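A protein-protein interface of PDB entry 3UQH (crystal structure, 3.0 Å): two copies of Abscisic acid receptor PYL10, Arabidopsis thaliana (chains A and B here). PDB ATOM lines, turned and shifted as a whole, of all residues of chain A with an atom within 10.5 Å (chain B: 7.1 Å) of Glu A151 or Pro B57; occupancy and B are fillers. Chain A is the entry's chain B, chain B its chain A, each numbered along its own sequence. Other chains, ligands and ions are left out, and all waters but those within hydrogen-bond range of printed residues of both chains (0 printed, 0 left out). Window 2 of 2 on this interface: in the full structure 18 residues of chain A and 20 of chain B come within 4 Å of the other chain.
The side-chain amino group (NZ) of Lys B80 lies within hydrogen-bond range of the backbone carbonyl oxygen (O) of Gly A146.
The backbone carbonyl oxygen of Pro B57 sits at hydrogen-bond distance from the side-chain amide nitrogen of Asn A147.
The side-chain sulfur (SG) of Cys A153 is disulfide-bonded to the side-chain sulfur (SG) of Cys A27.
The backbone carbonyl oxygen of Phe B58 sits at hydrogen-bond distance from the backbone NH of Lys B80.
The backbone carbonyl oxygen (O) of Glu A145 sits close to the side-chain amide oxygen (OD1) of Asn A147 (3.4 Å).
The backbone carbonyl oxygen (O) of Leu B159 lies close to the side-chain amide oxygen (OD1) of Asn B163.
The backbone NH (N) of Thr A148 lies within hydrogen-bond range of the side-chain carboxylate (OE1) of Glu A151, at 3.2 Å.
The side-chain amide nitrogen (ND2) of Asn A147 is in hydrogen-bond range of the side-chain carboxylate (OE1) of Glu A151 (3.3 Å).
Phe B58 touches Asn A147.
CD of Lys B80 touches ND2 of Asn A147 (3.8 Å).
CB of Pro B57 touches CD of Glu A151 (3.6 Å).
O of Glu A151 touches CZ of Phe B58, at 3.9 Å.
CE1 of Phe A154 touches CB of Ala B158, 3.5 Å away.
Phe B58 touches Phe A155 (CZ to CE1, 3.8 Å).
CZ of Phe A155 touches CA of Leu B159, 3.8 Å away.
Of the printed residues of chain B, Gly A146 touches Lys B80.
Glu A150 touches none of the printed residues of chain B.
Pro B57 touches just these residues of chain A: Asn A147 and Glu A151.
Phe B58 touches just these residues of chain A: Asn A147, Glu A151 and Phe A155.
Of the printed residues of chain A, Lys B80 touches Gly A146 and Asn A147.
Of the printed residues of chain A, Ala B158 touches Phe A154.
Asn B163 touches none of the printed residues of chain A.
Leu B164 touches none of the printed residues of chain A.
The nearest residue of chain B that does not touch Glu A151 is Cys B162 (4.2 Å).
The nearest printed residue of chain A that does not touch Leu B159 is Phe A154 (4.8 Å).
Of the 19 printed residues of chain B, 5 touch a printed residue of chain A.
Printed residues of chain B that touch a printed residue of chain A: Pro B57, Phe B58, Lys B80, Ala B158 and Leu B159.
Of the 18 printed residues of chain A, 5 touch a printed residue of chain B.
Hydrophobic or aromatic side chains of chain A within 4 Å of the printed part of chain B: Phe A154 and Phe A155.
Along chain A the printed residues that touch a printed residue of chain B span positions 146 to 155.
Among the printed residues, no Asp or Glu carboxylate lies within 4 Å of a Lys or Arg side-chain nitrogen of the other chain.
1 position is printed for both chains.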
ATOM      1  N   CYS A  27      29.554 -29.246   4.562  1.00  0.00           N
ATOM      2  CA  CYS A  27      28.400 -29.081   3.701  1.00  0.00           C
ATOM      3  C   CYS A  27      28.593 -29.261   2.208  1.00  0.00           C
ATOM      4  O   CYS A  27      29.452 -28.653   1.579  1.00  0.00           O
ATOM      5  CB  CYS A  27      27.616 -27.819   4.020  1.00  0.00           C
ATOM      6  SG  CYS A  27      28.382 -26.193   3.828  1.00  0.00           S
ATOM      7  N   ASP A 142      34.032 -27.752   4.507  1.00  0.00           N
ATOM      8  CA  ASP A 142      33.856 -27.809   5.948  1.00  0.00           C
ATOM      9  C   ASP A 142      33.166 -26.554   6.449  1.00  0.00           C
ATOM     10  O   ASP A 142      33.567 -25.438   6.102  1.00  0.00           O
ATOM     11  CB  ASP A 142      35.208 -27.966   6.633  1.00  0.00           C
ATOM     12  CG  ASP A 142      35.854 -29.302   6.333  1.00  0.00           C
ATOM     13  OD1 ASP A 142      35.306 -30.083   5.513  1.00  0.00           O
ATOM     14  OD2 ASP A 142      36.918 -29.579   6.923  1.00  0.00           O
ATOM     15  N   VAL A 143      32.159 -26.732   7.299  1.00  0.00           N
ATOM     16  CA  VAL A 143      31.525 -25.611   7.978  1.00  0.00           C
ATOM     17  C   VAL A 143      32.467 -25.090   9.058  1.00  0.00           C
ATOM     18  O   VAL A 143      32.938 -25.853   9.901  1.00  0.00           O
ATOM     19  CB  VAL A 143      30.188 -26.018   8.620  1.00  0.00           C
ATOM     20  CG1 VAL A 143      30.401 -27.149   9.614  1.00  0.00           C
ATOM     21  CG2 VAL A 143      29.538 -24.821   9.298  1.00  0.00           C
ATOM     22  N   PRO A 144      32.747 -23.791   9.024  1.00  0.00           N
ATOM     23  CA  PRO A 144      33.724 -23.189   9.936  1.00  0.00           C
ATOM     24  C   PRO A 144      33.425 -23.481  11.398  1.00  0.00           C
ATOM     25  O   PRO A 144      32.289 -23.791  11.757  1.00  0.00           O
ATOM     26  CB  PRO A 144      33.574 -21.690   9.660  1.00  0.00           C
ATOM     27  CG  PRO A 144      33.112 -21.619   8.248  1.00  0.00           C
ATOM     28  CD  PRO A 144      32.232 -22.821   8.043  1.00  0.00           C
ATOM     29  N   GLU A 145      34.444 -23.377  12.245  1.00  0.00           N
ATOM     30  CA  GLU A 145      34.278 -23.633  13.672  1.00  0.00           C
ATOM     31  C   GLU A 145      33.308 -22.642  14.311  1.00  0.00           C
ATOM     32  O   GLU A 145      33.413 -21.433  14.099  1.00  0.00           O
ATOM     33  CB  GLU A 145      35.630 -23.580  14.386  1.00  0.00           C
ATOM     34  CG  GLU A 145      36.792 -24.102  13.556  1.00  0.00           C
ATOM     35  CD  GLU A 145      38.048 -24.309  14.378  1.00  0.00           C
ATOM     36  OE1 GLU A 145      38.534 -23.328  14.981  1.00  0.00           O
ATOM     37  OE2 GLU A 145      38.551 -25.451  14.421  1.00  0.00           O
ATOM     38  N   GLY A 146      32.367 -23.159  15.095  1.00  0.00           N
ATOM     39  CA  GLY A 146      31.386 -22.315  15.781  1.00  0.00           C
ATOM     40  C   GLY A 146      30.239 -21.736  14.965  1.00  0.00           C
ATOM     41  O   GLY A 146      29.419 -20.997  15.501  1.00  0.00           O
ATOM     42  N   ASN A 147      30.165 -22.065  13.679  1.00  0.00           N
ATOM     43  CA  ASN A 147      29.044 -21.628  12.849  1.00  0.00           C
ATOM     44  C   ASN A 147      28.241 -22.793  12.295  1.00  0.00           C
ATOM     45  O   ASN A 147      28.810 -23.828  11.963  1.00  0.00           O
ATOM     46  CB  ASN A 147      29.542 -20.751  11.707  1.00  0.00           C
ATOM     47  CG  ASN A 147      30.179 -19.483  12.199  1.00  0.00           C
ATOM     48  OD1 ASN A 147      31.406 -19.381  12.273  1.00  0.00           O
ATOM     49  ND2 ASN A 147      29.351 -18.513  12.572  1.00  0.00           N
ATOM     50  N   THR A 148      26.925 -22.616  12.190  1.00  0.00           N
ATOM     51  CA  THR A 148      26.038 -23.680  11.717  1.00  0.00           C
ATOM     52  C   THR A 148      25.899 -23.667  10.202  1.00  0.00           C
ATOM     53  O   THR A 148      26.050 -22.622   9.572  1.00  0.00           O
ATOM     54  CB  THR A 148      24.612 -23.616  12.358  1.00  0.00           C
ATOM     55  OG1 THR A 148      23.865 -22.529  11.800  1.00  0.00           O
ATOM     56  CG2 THR A 148      24.674 -23.471  13.883  1.00  0.00           C
ATOM     57  N   LYS A 149      25.564 -24.834   9.585  1.00  0.00           N
ATOM     58  CA  LYS A 149      25.241 -24.980   8.160  1.00  0.00           C
ATOM     59  C   LYS A 149      24.281 -23.897   7.699  1.00  0.00           C
ATOM     60  O   LYS A 149      24.465 -23.302   6.629  1.00  0.00           O
ATOM     61  CB  LYS A 149      24.620 -26.357   7.891  1.00  0.00           C
ATOM     62  CG  LYS A 149      25.562 -27.514   8.138  1.00  0.00           C
ATOM     63  CD  LYS A 149      24.904 -28.868   7.858  1.00  0.00           C
ATOM     64  CE  LYS A 149      25.833 -30.034   8.153  1.00  0.00           C
ATOM     65  NZ  LYS A 149      25.778 -31.078   7.087  1.00  0.00           N
ATOM     66  N   GLU A 150      23.313 -23.639   8.572  1.00  0.00           N
ATOM     67  CA  GLU A 150      22.267 -22.670   8.248  1.00  0.00           C
ATOM     68  C   GLU A 150      22.791 -21.239   8.178  1.00  0.00           C
ATOM     69  O   GLU A 150      22.237 -20.413   7.448  1.00  0.00           O
ATOM     70  CB  GLU A 150      21.095 -22.791   9.222  1.00  0.00           C
ATOM     71  CG  GLU A 150      20.403 -24.153   9.166  1.00  0.00           C
ATOM     72  CD  GLU A 150      19.075 -24.176   9.906  1.00  0.00           C
ATOM     73  OE1 GLU A 150      18.759 -23.189  10.615  1.00  0.00           O
ATOM     74  OE2 GLU A 150      18.345 -25.187   9.779  1.00  0.00           O
ATOM     75  N   GLU A 151      23.873 -20.967   8.907  1.00  0.00           N
ATOM     76  CA  GLU A 151      24.542 -19.660   8.859  1.00  0.00           C
ATOM     77  C   GLU A 151      25.428 -19.592   7.636  1.00  0.00           C
ATOM     78  O   GLU A 151      25.421 -18.587   6.919  1.00  0.00           O
ATOM     79  CB  GLU A 151      25.240 -19.405  10.210  1.00  0.00           C
ATOM     80  CG  GLU A 151      24.300 -19.254  11.388  1.00  0.00           C
ATOM     81  CD  GLU A 151      24.984 -19.457  12.733  1.00  0.00           C
ATOM     82  OE1 GLU A 151      26.235 -19.509  12.802  1.00  0.00           O
ATOM     83  OE2 GLU A 151      24.257 -19.563  13.737  1.00  0.00           O
ATOM     84  N   THR A 152      26.178 -20.662   7.376  1.00  0.00           N
ATOM     85  CA  THR A 152      27.237 -20.622   6.343  1.00  0.00           C
ATOM     86  C   THR A 152      26.936 -20.957   4.908  1.00  0.00           C
ATOM     87  O   THR A 152      27.282 -20.169   4.032  1.00  0.00           O
ATOM     88  CB  THR A 152      28.362 -21.576   6.826  1.00  0.00           C
ATOM     89  OG1 THR A 152      27.805 -22.852   7.138  1.00  0.00           O
ATOM     90  CG2 THR A 152      29.069 -21.039   8.038  1.00  0.00           C
ATOM     91  N   CYS A 153      26.309 -22.105   4.642  1.00  0.00           N
ATOM     92  CA  CYS A 153      26.394 -22.722   3.303  1.00  0.00           C
ATOM     93  C   CYS A 153      25.649 -22.010   2.188  1.00  0.00           C
ATOM     94  O   CYS A 153      25.978 -22.189   1.016  1.00  0.00           O
ATOM     95  CB  CYS A 153      26.028 -24.210   3.339  1.00  0.00           C
ATOM     96  SG  CYS A 153      26.877 -25.082   4.675  1.00  0.00           S
ATOM     97  N   PHE A 154      24.666 -21.190   2.549  1.00  0.00           N
ATOM     98  CA  PHE A 154      23.971 -20.387   1.558  1.00  0.00           C
ATOM     99  C   PHE A 154      24.848 -19.288   0.963  1.00  0.00           C
ATOM    100  O   PHE A 154      24.535 -18.764  -0.097  1.00  0.00           O
ATOM    101  CB  PHE A 154      22.677 -19.810   2.116  1.00  0.00           C
ATOM    102  CG  PHE A 154      22.874 -18.683   3.081  1.00  0.00           C
ATOM    103  CD1 PHE A 154      23.340 -17.442   2.641  1.00  0.00           C
ATOM    104  CD2 PHE A 154      22.544 -18.845   4.431  1.00  0.00           C
ATOM    105  CE1 PHE A 154      23.510 -16.387   3.532  1.00  0.00           C
ATOM    106  CE2 PHE A 154      22.701 -17.796   5.339  1.00  0.00           C
ATOM    107  CZ  PHE A 154      23.190 -16.560   4.889  1.00  0.00           C
ATOM    108  N   PHE A 155      25.935 -18.933   1.642  1.00  0.00           N
ATOM    109  CA  PHE A 155      26.927 -18.017   1.063  1.00  0.00           C
ATOM    110  C   PHE A 155      27.694 -18.716  -0.052  1.00  0.00           C
ATOM    111  O   PHE A 155      27.892 -18.139  -1.124  1.00  0.00           O
ATOM    112  CB  PHE A 155      27.913 -17.482   2.116  1.00  0.00           C
ATOM    113  CG  PHE A 155      27.326 -16.457   3.040  1.00  0.00           C
ATOM    114  CD1 PHE A 155      27.203 -16.723   4.403  1.00  0.00           C
ATOM    115  CD2 PHE A 155      26.891 -15.227   2.554  1.00  0.00           C
ATOM    116  CE1 PHE A 155      26.658 -15.783   5.268  1.00  0.00           C
ATOM    117  CE2 PHE A 155      26.336 -14.281   3.413  1.00  0.00           C
ATOM    118  CZ  PHE A 155      26.221 -14.560   4.774  1.00  0.00           C
ATOM    119  N   VAL A 156      28.121 -19.955   0.196  1.00  0.00           N
ATOM    120  CA  VAL A 156      28.873 -20.704  -0.811  1.00  0.00           C
ATOM    121  C   VAL A 156      27.960 -21.077  -1.978  1.00  0.00           C
ATOM    122  O   VAL A 156      28.375 -21.001  -3.133  1.00  0.00           O
ATOM    123  CB  VAL A 156      29.589 -21.946  -0.243  1.00  0.00           C
ATOM    124  CG1 VAL A 156      30.595 -22.478  -1.254  1.00  0.00           C
ATOM    125  CG2 VAL A 156      30.307 -21.604   1.048  1.00  0.00           C
ATOM    126  N   GLU A 157      26.714 -21.445  -1.679  1.00  0.00           N
ATOM    127  CA  GLU A 157      25.706 -21.676  -2.726  1.00  0.00           C
ATOM    128  C   GLU A 157      25.479 -20.424  -3.579  1.00  0.00           C
ATOM    129  O   GLU A 157      25.316 -20.516  -4.802  1.00  0.00           O
ATOM    130  CB  GLU A 157      24.388 -22.138  -2.119  1.00  0.00           C
ATOM    131  CG  GLU A 157      24.384 -23.582  -1.695  1.00  0.00           C
ATOM    132  CD  GLU A 157      23.289 -23.910  -0.688  1.00  0.00           C
ATOM    133  OE1 GLU A 157      22.310 -23.145  -0.561  1.00  0.00           O
ATOM    134  OE2 GLU A 157      23.405 -24.948  -0.011  1.00  0.00           O
ATOM    135  N   ALA A 158      25.473 -19.266  -2.926  1.00  0.00           N
ATOM    136  CA  ALA A 158      25.252 -17.998  -3.608  1.00  0.00           C
ATOM    137  C   ALA A 158      26.378 -17.681  -4.585  1.00  0.00           C
ATOM    138  O   ALA A 158      26.128 -17.359  -5.747  1.00  0.00           O
ATOM    139  CB  ALA A 158      25.094 -16.873  -2.594  1.00  0.00           C
ATOM    140  N   PRO B  52      26.960  -7.310  20.359  1.00  0.00           N
ATOM    141  CA  PRO B  52      26.215  -7.815  19.218  1.00  0.00           C
ATOM    142  C   PRO B  52      26.301  -9.350  19.114  1.00  0.00           C
ATOM    143  O   PRO B  52      25.566  -9.948  18.326  1.00  0.00           O
ATOM    144  CB  PRO B  52      26.885  -7.129  18.032  1.00  0.00           C
ATOM    145  CG  PRO B  52      28.241  -6.828  18.485  1.00  0.00           C
ATOM    146  CD  PRO B  52      28.166  -6.571  19.947  1.00  0.00           C
ATOM    147  N   GLN B  53      27.175  -9.973  19.913  1.00  0.00           N
ATOM    148  CA  GLN B  53      27.262 -11.439  20.016  1.00  0.00           C
ATOM    149  C   GLN B  53      25.957 -12.057  20.498  1.00  0.00           C
ATOM    150  O   GLN B  53      25.676 -13.217  20.206  1.00  0.00           O
ATOM    151  CB  GLN B  53      28.321 -11.872  21.031  1.00  0.00           C
ATOM    152  CG  GLN B  53      29.735 -11.531  20.702  1.00  0.00           C
ATOM    153  CD  GLN B  53      30.103 -10.131  21.135  1.00  0.00           C
ATOM    154  OE1 GLN B  53      29.287  -9.399  21.694  1.00  0.00           O
ATOM    155  NE2 GLN B  53      31.343  -9.752  20.877  1.00  0.00           N
ATOM    156  N   LYS B  54      25.187 -11.301  21.272  1.00  0.00           N
ATOM    157  CA  LYS B  54      23.959 -11.820  21.856  1.00  0.00           C
ATOM    158  C   LYS B  54      23.084 -12.476  20.797  1.00  0.00           C
ATOM    159  O   LYS B  54      22.486 -13.528  21.057  1.00  0.00           O
ATOM    160  CB  LYS B  54      23.194 -10.722  22.592  1.00  0.00           C
ATOM    161  CG  LYS B  54      23.365 -10.735  24.116  1.00  0.00           C
ATOM    162  CD  LYS B  54      22.670  -9.506  24.713  1.00  0.00           C
ATOM    163  CE  LYS B  54      22.348  -9.628  26.209  1.00  0.00           C
ATOM    164  NZ  LYS B  54      21.649  -8.379  26.660  1.00  0.00           N
ATOM    165  N   TYR B  55      23.034 -11.870  19.607  1.00  0.00           N
ATOM    166  CA  TYR B  55      22.300 -12.447  18.481  1.00  0.00           C
ATOM    167  C   TYR B  55      23.042 -12.561  17.129  1.00  0.00           C
ATOM    168  O   TYR B  55      22.695 -13.426  16.334  1.00  0.00           O
ATOM    169  CB  TYR B  55      20.952 -11.748  18.307  1.00  0.00           C
ATOM    170  CG  TYR B  55      21.003 -10.446  17.543  1.00  0.00           C
ATOM    171  CD1 TYR B  55      20.719 -10.410  16.172  1.00  0.00           C
ATOM    172  CD2 TYR B  55      21.320  -9.242  18.187  1.00  0.00           C
ATOM    173  CE1 TYR B  55      20.752  -9.210  15.451  1.00  0.00           C
ATOM    174  CE2 TYR B  55      21.349  -8.029  17.477  1.00  0.00           C
ATOM    175  CZ  TYR B  55      21.066  -8.024  16.108  1.00  0.00           C
ATOM    176  OH  TYR B  55      21.095  -6.838  15.403  1.00  0.00           O
ATOM    177  N   LYS B  56      24.036 -11.710  16.854  1.00  0.00           N
ATOM    178  CA  LYS B  56      24.756 -11.786  15.562  1.00  0.00           C
ATOM    179  C   LYS B  56      25.724 -12.977  15.490  1.00  0.00           C
ATOM    180  O   LYS B  56      26.611 -13.117  16.343  1.00  0.00           O
ATOM    181  CB  LYS B  56      25.491 -10.495  15.249  1.00  0.00           C
ATOM    182  CG  LYS B  56      24.595  -9.285  15.143  1.00  0.00           C
ATOM    183  CD  LYS B  56      25.331  -8.163  14.454  1.00  0.00           C
ATOM    184  CE  LYS B  56      24.542  -6.885  14.509  1.00  0.00           C
ATOM    185  NZ  LYS B  56      25.353  -5.729  14.002  1.00  0.00           N
ATOM    186  N   PRO B  57      25.554 -13.850  14.479  1.00  0.00           N
ATOM    187  CA  PRO B  57      26.235 -15.145  14.550  1.00  0.00           C
ATOM    188  C   PRO B  57      27.713 -15.224  14.115  1.00  0.00           C
ATOM    189  O   PRO B  57      28.345 -16.266  14.329  1.00  0.00           O
ATOM    190  CB  PRO B  57      25.351 -16.052  13.687  1.00  0.00           C
ATOM    191  CG  PRO B  57      24.729 -15.139  12.712  1.00  0.00           C
ATOM    192  CD  PRO B  57      24.538 -13.826  13.414  1.00  0.00           C
ATOM    193  N   PHE B  58      28.282 -14.177  13.534  1.00  0.00           N
ATOM    194  CA  PHE B  58      29.671 -14.323  13.107  1.00  0.00           C
ATOM    195  C   PHE B  58      30.690 -13.739  14.075  1.00  0.00           C
ATOM    196  O   PHE B  58      31.905 -13.849  13.863  1.00  0.00           O
ATOM    197  CB  PHE B  58      29.855 -13.829  11.682  1.00  0.00           C
ATOM    198  CG  PHE B  58      28.981 -14.541  10.719  1.00  0.00           C
ATOM    199  CD1 PHE B  58      29.153 -15.899  10.490  1.00  0.00           C
ATOM    200  CD2 PHE B  58      27.947 -13.874  10.078  1.00  0.00           C
ATOM    201  CE1 PHE B  58      28.323 -16.579   9.614  1.00  0.00           C
ATOM    202  CE2 PHE B  58      27.109 -14.544   9.201  1.00  0.00           C
ATOM    203  CZ  PHE B  58      27.299 -15.900   8.971  1.00  0.00           C
ATOM    204  N   ILE B  59      30.180 -13.175  15.164  1.00  0.00           N
ATOM    205  CA  ILE B  59      30.979 -12.350  16.054  1.00  0.00           C
ATOM    206  C   ILE B  59      31.537 -13.134  17.231  1.00  0.00           C
ATOM    207  O   ILE B  59      30.803 -13.806  17.949  1.00  0.00           O
ATOM    208  CB  ILE B  59      30.188 -11.105  16.498  1.00  0.00           C
ATOM    209  CG1 ILE B  59      29.860 -10.256  15.261  1.00  0.00           C
ATOM    210  CG2 ILE B  59      30.958 -10.297  17.533  1.00  0.00           C
ATOM    211  CD1 ILE B  59      29.009  -9.053  15.546  1.00  0.00           C
ATOM    212  N   SER B  60      32.851 -13.031  17.397  1.00  0.00           N
ATOM    213  CA  SER B  60      33.612 -13.717  18.434  1.00  0.00           C
ATOM    214  C   SER B  60      33.893 -12.834  19.675  1.00  0.00           C
ATOM    215  O   SER B  60      33.768 -13.291  20.816  1.00  0.00           O
ATOM    216  CB  SER B  60      34.917 -14.212  17.815  1.00  0.00           C
ATOM    217  OG  SER B  60      35.869 -14.544  18.800  1.00  0.00           O
ATOM    218  N   LEU B  79      35.586 -11.117  14.295  1.00  0.00           N
ATOM    219  CA  LEU B  79      34.824 -12.219  13.734  1.00  0.00           C
ATOM    220  C   LEU B  79      35.370 -13.543  14.246  1.00  0.00           C
ATOM    221  O   LEU B  79      36.477 -13.602  14.780  1.00  0.00           O
ATOM    222  CB  LEU B  79      34.853 -12.154  12.210  1.00  0.00           C
ATOM    223  CG  LEU B  79      34.224 -10.870  11.657  1.00  0.00           C
ATOM    224  CD1 LEU B  79      34.534 -10.663  10.198  1.00  0.00           C
ATOM    225  CD2 LEU B  79      32.736 -10.862  11.872  1.00  0.00           C
ATOM    226  N   LYS B  80      34.581 -14.602  14.106  1.00  0.00           N
ATOM    227  CA  LYS B  80      35.015 -15.942  14.481  1.00  0.00           C
ATOM    228  C   LYS B  80      36.034 -16.455  13.465  1.00  0.00           C
ATOM    229  O   LYS B  80      36.187 -15.883  12.386  1.00  0.00           O
ATOM    230  CB  LYS B  80      33.809 -16.872  14.559  1.00  0.00           C
ATOM    231  CG  LYS B  80      32.856 -16.573  15.710  1.00  0.00           C
ATOM    232  CD  LYS B  80      31.462 -17.119  15.437  1.00  0.00           C
ATOM    233  CE  LYS B  80      30.751 -17.489  16.727  1.00  0.00           C
ATOM    234  NZ  LYS B  80      29.338 -17.878  16.479  1.00  0.00           N
ATOM    235  N   LEU B  83      36.448 -17.431   8.627  1.00  0.00           N
ATOM    236  CA  LEU B  83      35.620 -16.605   7.745  1.00  0.00           C
ATOM    237  C   LEU B  83      36.471 -15.669   6.876  1.00  0.00           C
ATOM    238  O   LEU B  83      37.596 -15.325   7.253  1.00  0.00           O
ATOM    239  CB  LEU B  83      34.604 -15.796   8.561  1.00  0.00           C
ATOM    240  CG  LEU B  83      33.709 -16.502   9.588  1.00  0.00           C
ATOM    241  CD1 LEU B  83      32.939 -15.473  10.419  1.00  0.00           C
ATOM    242  CD2 LEU B  83      32.763 -17.483   8.917  1.00  0.00           C
ATOM    243  N   ALA B 158      21.655 -11.060   2.533  1.00  0.00           N
ATOM    244  CA  ALA B 158      21.610 -12.384   3.098  1.00  0.00           C
ATOM    245  C   ALA B 158      22.216 -12.396   4.482  1.00  0.00           C
ATOM    246  O   ALA B 158      21.625 -12.944   5.399  1.00  0.00           O
ATOM    247  CB  ALA B 158      22.286 -13.376   2.191  1.00  0.00           C
ATOM    248  N   LEU B 159      23.369 -11.767   4.657  1.00  0.00           N
ATOM    249  CA  LEU B 159      23.969 -11.705   5.993  1.00  0.00           C
ATOM    250  C   LEU B 159      23.022 -11.058   6.990  1.00  0.00           C
ATOM    251  O   LEU B 159      22.948 -11.478   8.141  1.00  0.00           O
ATOM    252  CB  LEU B 159      25.297 -10.953   5.991  1.00  0.00           C
ATOM    253  CG  LEU B 159      26.004 -10.842   7.348  1.00  0.00           C
ATOM    254  CD1 LEU B 159      27.430 -11.262   7.196  1.00  0.00           C
ATOM    255  CD2 LEU B 159      25.940  -9.443   7.903  1.00  0.00           C
ATOM    256  N   CYS B 162      20.214 -13.134   7.767  1.00  0.00           N
ATOM    257  CA  CYS B 162      20.805 -14.098   8.681  1.00  0.00           C
ATOM    258  C   CYS B 162      20.780 -13.615  10.137  1.00  0.00           C
ATOM    259  O   CYS B 162      20.415 -14.373  11.036  1.00  0.00           O
ATOM    260  CB  CYS B 162      22.224 -14.431   8.233  1.00  0.00           C
ATOM    261  SG  CYS B 162      22.996 -15.780   9.128  1.00  0.00           S
ATOM    262  N   ASN B 163      21.145 -12.351  10.360  1.00  0.00           N
ATOM    263  CA  ASN B 163      21.129 -11.763  11.700  1.00  0.00           C
ATOM    264  C   ASN B 163      19.717 -11.603  12.195  1.00  0.00           C
ATOM    265  O   ASN B 163      19.456 -11.786  13.381  1.00  0.00           O
ATOM    266  CB  ASN B 163      21.784 -10.383  11.740  1.00  0.00           C
ATOM    267  CG  ASN B 163      23.207 -10.382  11.249  1.00  0.00           C
ATOM    268  OD1 ASN B 163      23.868 -11.515  11.300  1.00  0.00           O
ATOM    269  ND2 ASN B 163      23.707  -9.356  10.835  1.00  0.00           N
ATOM    270  N   LEU B 164      18.810 -11.241  11.293  1.00  0.00           N
ATOM    271  CA  LEU B 164      17.418 -11.051  11.667  1.00  0.00           C
ATOM    272  C   LEU B 164      16.786 -12.379  12.059  1.00  0.00           C
ATOM    273  O   LEU B 164      16.127 -12.472  13.088  1.00  0.00           O
ATOM    274  CB  LEU B 164      16.623 -10.354  10.558  1.00  0.00           C
ATOM    275  CG  LEU B 164      16.891  -8.856  10.358  1.00  0.00           C
ATOM    276  CD1 LEU B 164      15.990  -8.254   9.280  1.00  0.00           C
ATOM    277  CD2 LEU B 164      16.784  -8.042  11.664  1.00  0.00           C
ATOM    278  N   SER B 166      18.298 -14.926  13.127  1.00  0.00           N
ATOM    279  CA  SER B 166      18.950 -15.287  14.366  1.00  0.00           C
ATOM    280  C   SER B 166      18.364 -14.527  15.550  1.00  0.00           C
ATOM    281  O   SER B 166      18.142 -15.097  16.622  1.00  0.00           O
ATOM    282  CB  SER B 166      20.434 -15.014  14.267  1.00  0.00           C
ATOM    283  OG  SER B 166      20.956 -14.863  15.564  1.00  0.00           O
ATOM    284  N   LEU B 167      18.121 -13.239  15.349  1.00  0.00           N
ATOM    285  CA  LEU B 167      17.468 -12.429  16.360  1.00  0.00           C
ATOM    286  C   LEU B 167      16.144 -13.057  16.774  1.00  0.00           C
ATOM    287  O   LEU B 167      15.860 -13.159  17.960  1.00  0.00           O
ATOM    288  CB  LEU B 167      17.252 -11.004  15.861  1.00  0.00           C
ATOM    289  CG  LEU B 167      16.555 -10.015  16.791  1.00  0.00           C
ATOM    290  CD1 LEU B 167      17.304  -9.851  18.103  1.00  0.00           C
ATOM    291  CD2 LEU B 167      16.419  -8.695  16.078  1.00  0.00           C
